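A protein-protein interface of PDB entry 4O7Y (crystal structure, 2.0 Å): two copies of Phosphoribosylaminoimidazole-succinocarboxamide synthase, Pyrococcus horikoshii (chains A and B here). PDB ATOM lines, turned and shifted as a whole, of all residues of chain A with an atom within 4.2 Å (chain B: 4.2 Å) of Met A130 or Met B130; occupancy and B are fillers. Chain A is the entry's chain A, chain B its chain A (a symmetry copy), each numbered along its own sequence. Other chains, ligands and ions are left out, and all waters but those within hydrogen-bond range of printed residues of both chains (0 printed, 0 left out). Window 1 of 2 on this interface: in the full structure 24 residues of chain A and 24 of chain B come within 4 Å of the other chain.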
ATOM      1  N   ARG A 103      -3.163  19.505  21.629  1.00  0.00           N
ATOM      2  CA  ARG A 103      -2.303  18.700  22.466  1.00  0.00           C
ATOM      3  C   ARG A 103      -2.577  18.988  23.949  1.00  0.00           C
ATOM      4  O   ARG A 103      -2.482  18.087  24.776  1.00  0.00           O
ATOM      5  CB  ARG A 103      -0.844  18.967  22.093  1.00  0.00           C
ATOM      6  CG  ARG A 103       0.083  17.789  22.276  1.00  0.00           C
ATOM      7  CD  ARG A 103       1.502  18.113  21.836  1.00  0.00           C
ATOM      8  NE  ARG A 103       1.687  18.123  20.382  1.00  0.00           N
ATOM      9  CZ  ARG A 103       1.727  17.024  19.619  1.00  0.00           C
ATOM     10  NH1 ARG A 103       1.554  15.806  20.137  1.00  0.00           N
ATOM     11  NH2 ARG A 103       1.916  17.139  18.312  1.00  0.00           N
ATOM     12  N   LEU A 119      10.059  19.175  19.923  1.00  0.00           N
ATOM     13  CA  LEU A 119      10.928  18.652  18.859  1.00  0.00           C
ATOM     14  C   LEU A 119      10.081  17.931  17.837  1.00  0.00           C
ATOM     15  O   LEU A 119       9.257  17.109  18.232  1.00  0.00           O
ATOM     16  CB  LEU A 119      11.942  17.659  19.426  1.00  0.00           C
ATOM     17  CG  LEU A 119      12.752  18.247  20.597  1.00  0.00           C
ATOM     18  CD1 LEU A 119      13.572  17.179  21.314  1.00  0.00           C
ATOM     19  CD2 LEU A 119      13.634  19.395  20.085  1.00  0.00           C
ATOM     20  N   TYR A 120      10.319  18.230  16.550  1.00  0.00           N
ATOM     21  CA  TYR A 120       9.629  17.591  15.421  1.00  0.00           C
ATOM     22  C   TYR A 120      10.693  16.966  14.518  1.00  0.00           C
ATOM     23  O   TYR A 120      11.700  17.583  14.218  1.00  0.00           O
ATOM     24  CB  TYR A 120       8.773  18.573  14.609  1.00  0.00           C
ATOM     25  CG  TYR A 120       7.577  19.056  15.384  1.00  0.00           C
ATOM     26  CD1 TYR A 120       6.352  18.394  15.299  1.00  0.00           C
ATOM     27  CD2 TYR A 120       7.690  20.149  16.244  1.00  0.00           C
ATOM     28  CE1 TYR A 120       5.252  18.808  16.058  1.00  0.00           C
ATOM     29  CE2 TYR A 120       6.598  20.588  16.985  1.00  0.00           C
ATOM     30  CZ  TYR A 120       5.380  19.912  16.885  1.00  0.00           C
ATOM     31  OH  TYR A 120       4.308  20.343  17.646  1.00  0.00           O
ATOM     32  N   ASP A 128       6.485  15.126   9.430  1.00  0.00           N
ATOM     33  CA  ASP A 128       7.156  15.792  10.559  1.00  0.00           C
ATOM     34  C   ASP A 128       6.548  15.478  11.919  1.00  0.00           C
ATOM     35  O   ASP A 128       5.999  16.360  12.536  1.00  0.00           O
ATOM     36  CB  ASP A 128       7.166  17.290  10.358  1.00  0.00           C
ATOM     37  CG  ASP A 128       7.784  17.696   9.038  1.00  0.00           C
ATOM     38  OD1 ASP A 128       8.626  16.973   8.483  1.00  0.00           O
ATOM     39  OD2 ASP A 128       7.402  18.750   8.550  1.00  0.00           O
ATOM     40  N   PRO A 129       6.670  14.219  12.390  1.00  0.00           N
ATOM     41  CA  PRO A 129       5.977  13.935  13.637  1.00  0.00           C
ATOM     42  C   PRO A 129       6.764  14.511  14.816  1.00  0.00           C
ATOM     43  O   PRO A 129       8.005  14.666  14.739  1.00  0.00           O
ATOM     44  CB  PRO A 129       5.958  12.402  13.691  1.00  0.00           C
ATOM     45  CG  PRO A 129       7.155  11.988  12.871  1.00  0.00           C
ATOM     46  CD  PRO A 129       7.214  13.004  11.762  1.00  0.00           C
ATOM     47  N   MET A 130       6.044  14.814  15.891  1.00  0.00           N
ATOM     48  CA  MET A 130       6.691  15.239  17.117  1.00  0.00           C
ATOM     49  C   MET A 130       7.477  14.066  17.685  1.00  0.00           C
ATOM     50  O   MET A 130       7.065  12.912  17.567  1.00  0.00           O
ATOM     51  CB  MET A 130       5.663  15.729  18.144  1.00  0.00           C
ATOM     52  CG  MET A 130       6.319  16.623  19.197  1.00  0.00           C
ATOM     53  SD  MET A 130       5.221  17.291  20.500  1.00  0.00           S
ATOM     54  CE  MET A 130       4.961  15.841  21.494  1.00  0.00           C
ATOM     55  N   ILE A 131       8.615  14.356  18.302  1.00  0.00           N
ATOM     56  CA  ILE A 131       9.409  13.310  18.901  1.00  0.00           C
ATOM     57  C   ILE A 131       9.862  13.728  20.287  1.00  0.00           C
ATOM     58  O   ILE A 131       9.726  14.894  20.668  1.00  0.00           O
ATOM     59  CB  ILE A 131      10.651  12.934  18.039  1.00  0.00           C
ATOM     60  CG1 ILE A 131      11.498  14.178  17.717  1.00  0.00           C
ATOM     61  CG2 ILE A 131      10.192  12.132  16.808  1.00  0.00           C
ATOM     62  CD1 ILE A 131      12.937  13.854  17.299  1.00  0.00           C
ATOM     63  N   HIS A 135      13.461   9.323  21.001  1.00  0.00           N
ATOM     64  CA  HIS A 135      13.390   9.107  19.547  1.00  0.00           C
ATOM     65  C   HIS A 135      14.598   9.774  18.932  1.00  0.00           C
ATOM     66  O   HIS A 135      15.182   9.240  17.989  1.00  0.00           O
ATOM     67  CB  HIS A 135      12.139   9.710  18.891  1.00  0.00           C
ATOM     68  CG  HIS A 135      10.815   9.346  19.555  1.00  0.00           C
ATOM     69  ND1 HIS A 135      10.233   8.142  19.415  1.00  0.00           N
ATOM     70  CD2 HIS A 135       9.956  10.099  20.312  1.00  0.00           C
ATOM     71  CE1 HIS A 135       9.073   8.126  20.086  1.00  0.00           C
ATOM     72  NE2 HIS A 135       8.904   9.334  20.629  1.00  0.00           N
ATOM     73  N   ARG B 103       6.238   7.248  13.472  1.00  0.00           N
ATOM     74  CA  ARG B 103       6.988   8.311  14.101  1.00  0.00           C
ATOM     75  C   ARG B 103       8.472   8.218  13.721  1.00  0.00           C
ATOM     76  O   ARG B 103       9.135   9.241  13.585  1.00  0.00           O
ATOM     77  CB  ARG B 103       6.781   8.246  15.615  1.00  0.00           C
ATOM     78  CG  ARG B 103       6.828   9.581  16.320  1.00  0.00           C
ATOM     79  CD  ARG B 103       6.562   9.442  17.810  1.00  0.00           C
ATOM     80  NE  ARG B 103       5.151   9.235  18.148  1.00  0.00           N
ATOM     81  CZ  ARG B 103       4.214  10.190  18.093  1.00  0.00           C
ATOM     82  NH1 ARG B 103       4.499  11.426  17.677  1.00  0.00           N
ATOM     83  NH2 ARG B 103       2.966   9.904  18.435  1.00  0.00           N
ATOM     84  N   LEU B 119       5.532   9.589  26.581  1.00  0.00           N
ATOM     85  CA  LEU B 119       4.465  10.081  27.464  1.00  0.00           C
ATOM     86  C   LEU B 119       3.271  10.474  26.627  1.00  0.00           C
ATOM     87  O   LEU B 119       3.452  11.192  25.646  1.00  0.00           O
ATOM     88  CB  LEU B 119       4.928  11.311  28.243  1.00  0.00           C
ATOM     89  CG  LEU B 119       6.243  11.064  29.009  1.00  0.00           C
ATOM     90  CD1 LEU B 119       6.825  12.357  29.569  1.00  0.00           C
ATOM     91  CD2 LEU B 119       6.007  10.020  30.109  1.00  0.00           C
ATOM     92  N   TYR B 120       2.077  10.021  27.043  1.00  0.00           N
ATOM     93  CA  TYR B 120       0.805  10.345  26.384  1.00  0.00           C
ATOM     94  C   TYR B 120      -0.107  10.994  27.426  1.00  0.00           C
ATOM     95  O   TYR B 120      -0.217  10.522  28.543  1.00  0.00           O
ATOM     96  CB  TYR B 120       0.112   9.113  25.784  1.00  0.00           C
ATOM     97  CG  TYR B 120       0.863   8.560  24.604  1.00  0.00           C
ATOM     98  CD1 TYR B 120       0.569   8.978  23.307  1.00  0.00           C
ATOM     99  CD2 TYR B 120       1.905   7.652  24.797  1.00  0.00           C
ATOM    100  CE1 TYR B 120       1.301   8.505  22.212  1.00  0.00           C
ATOM    101  CE2 TYR B 120       2.624   7.153  23.717  1.00  0.00           C
ATOM    102  CZ  TYR B 120       2.314   7.583  22.424  1.00  0.00           C
ATOM    103  OH  TYR B 120       3.053   7.099  21.360  1.00  0.00           O
ATOM    104  N   ASP B 128      -5.748  11.251  23.540  1.00  0.00           N
ATOM    105  CA  ASP B 128      -4.473  10.899  24.185  1.00  0.00           C
ATOM    106  C   ASP B 128      -3.239  11.313  23.395  1.00  0.00           C
ATOM    107  O   ASP B 128      -2.523  10.458  22.930  1.00  0.00           O
ATOM    108  CB  ASP B 128      -4.409   9.412  24.453  1.00  0.00           C
ATOM    109  CG  ASP B 128      -5.588   8.916  25.262  1.00  0.00           C
ATOM    110  OD1 ASP B 128      -6.192   9.677  26.034  1.00  0.00           O
ATOM    111  OD2 ASP B 128      -5.914   7.748  25.105  1.00  0.00           O
ATOM    112  N   PRO B 129      -2.984  12.632  23.267  1.00  0.00           N
ATOM    113  CA  PRO B 129      -1.864  12.985  22.410  1.00  0.00           C
ATOM    114  C   PRO B 129      -0.545  12.748  23.149  1.00  0.00           C
ATOM    115  O   PRO B 129      -0.498  12.799  24.400  1.00  0.00           O
ATOM    116  CB  PRO B 129      -2.077  14.481  22.144  1.00  0.00           C
ATOM    117  CG  PRO B 129      -2.861  14.961  23.340  1.00  0.00           C
ATOM    118  CD  PRO B 129      -3.770  13.809  23.675  1.00  0.00           C
ATOM    119  N   MET B 130       0.507  12.498  22.376  1.00  0.00           N
ATOM    120  CA  MET B 130       1.834  12.390  22.949  1.00  0.00           C
ATOM    121  C   MET B 130       2.250  13.756  23.476  1.00  0.00           C
ATOM    122  O   MET B 130       1.903  14.788  22.903  1.00  0.00           O
ATOM    123  CB  MET B 130       2.848  11.898  21.910  1.00  0.00           C
ATOM    124  CG  MET B 130       4.087  11.308  22.584  1.00  0.00           C
ATOM    125  SD  MET B 130       5.397  10.675  21.473  1.00  0.00           S
ATOM    126  CE  MET B 130       6.102  12.196  20.885  1.00  0.00           C
ATOM    127  N   ILE B 131       2.994  13.769  24.575  1.00  0.00           N
ATOM    128  CA  ILE B 131       3.463  15.017  25.126  1.00  0.00           C
ATOM    129  C   ILE B 131       4.932  14.908  25.490  1.00  0.00           C
ATOM    130  O   ILE B 131       5.496  13.811  25.500  1.00  0.00           O
ATOM    131  CB  ILE B 131       2.648  15.462  26.377  1.00  0.00           C
ATOM    132  CG1 ILE B 131       2.613  14.348  27.439  1.00  0.00           C
ATOM    133  CG2 ILE B 131       1.265  15.968  25.929  1.00  0.00           C
ATOM    134  CD1 ILE B 131       2.258  14.847  28.845  1.00  0.00           C
ATOM    135  N   HIS B 135       5.149  19.927  28.254  1.00  0.00           N
ATOM    136  CA  HIS B 135       3.679  19.895  28.304  1.00  0.00           C
ATOM    137  C   HIS B 135       3.284  19.359  29.660  1.00  0.00           C
ATOM    138  O   HIS B 135       2.312  19.830  30.248  1.00  0.00           O
ATOM    139  CB  HIS B 135       3.042  18.988  27.240  1.00  0.00           C
ATOM    140  CG  HIS B 135       3.528  19.218  25.812  1.00  0.00           C
ATOM    141  ND1 HIS B 135       3.137  20.265  25.065  1.00  0.00           N
ATOM    142  CD2 HIS B 135       4.335  18.456  25.008  1.00  0.00           C
ATOM    143  CE1 HIS B 135       3.703  20.186  23.854  1.00  0.00           C
ATOM    144  NE2 HIS B 135       4.432  19.068  23.820  1.00  0.00           N
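Of the 8 printed residues of chain B, 4 touch a printed residue of chain A.
Hydrophobic or aromatic side chains of chain A that line the printed part of chain B: Pro A129, Met A130 and His A135.
SD of Met B130 lies close to NE of Arg B103 (3.6 Å).
NE of Arg A103 lies close to SD of Met A130 (3.6 Å).
NH1 of Arg A103 is in hydrogen-bond range of O of Met B130 (3.0 Å).
The backbone carbonyl oxygen (O) of Met A130 sits at hydrogen-bond distance from the guanidinium group (NH1) of Arg B103 (3.0 Å).
Arg A103 touches Pro B129.
His B135 touches Arg A103 (CE1 to CD, 3.6 Å).
Arg B103 touches Pro A129 (O to CG, 3.5 Å).
CE of Met A130 touches O of Met B130, at 3.5 Å.
SD of Met A130 touches NE2 of His B135 (3.8 Å).
CD of Arg B103 touches CE1 of His A135, 3.6 Å away.
SD of Met B130 touches NE2 of His A135, at 3.8 Å.
Arg A103 touches Pro B129, and with the chains exchanged Pro A129 touches Arg B103.
Arg A103 touches Met B130, and with the chains exchanged Met A130 touches Arg B103.
Arg A103 touches His B135, and with the chains exchanged His A135 touches Arg B103.
Met B130 touches its own counterpart, Met A130.
Of the 9 pairs that touch across the chains among the printed residues, 9 have their exchanged pair printed and touching as well.
Of the printed residues of chain B, Met A130 touches Arg B103, Met B130 and His B135.
Of the printed residues of chain A, Met B130 touches Arg A103, Met A130 and His A135.
Printed residues of chain B within 4 Å of Arg A103: Pro B129 (3.5 Å), Met B130 (3.0 Å) and His B135 (3.6 Å).
Printed residues of chain B within 4 Å of Pro A129: Arg B103.
Of the printed residues of chain A, Pro B129 touches Arg A103 (3.5 Å).
Of the printed residues of chain A, His B135 touches Arg A103 and Met A130.
Of the printed residues of chain B, His A135 touches Arg B103 and Met B130.
Tyr A120 touches none of the printed residues of chain B.
Asp A128 touches none of the printed residues of chain B.
The nearest printed residue of chain B that does not touch Met A130 is Ile B131 (4.01 Å).
The nearest printed residue of chain A that does not touch Met B130 is Ile A131 (4.01 Å).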
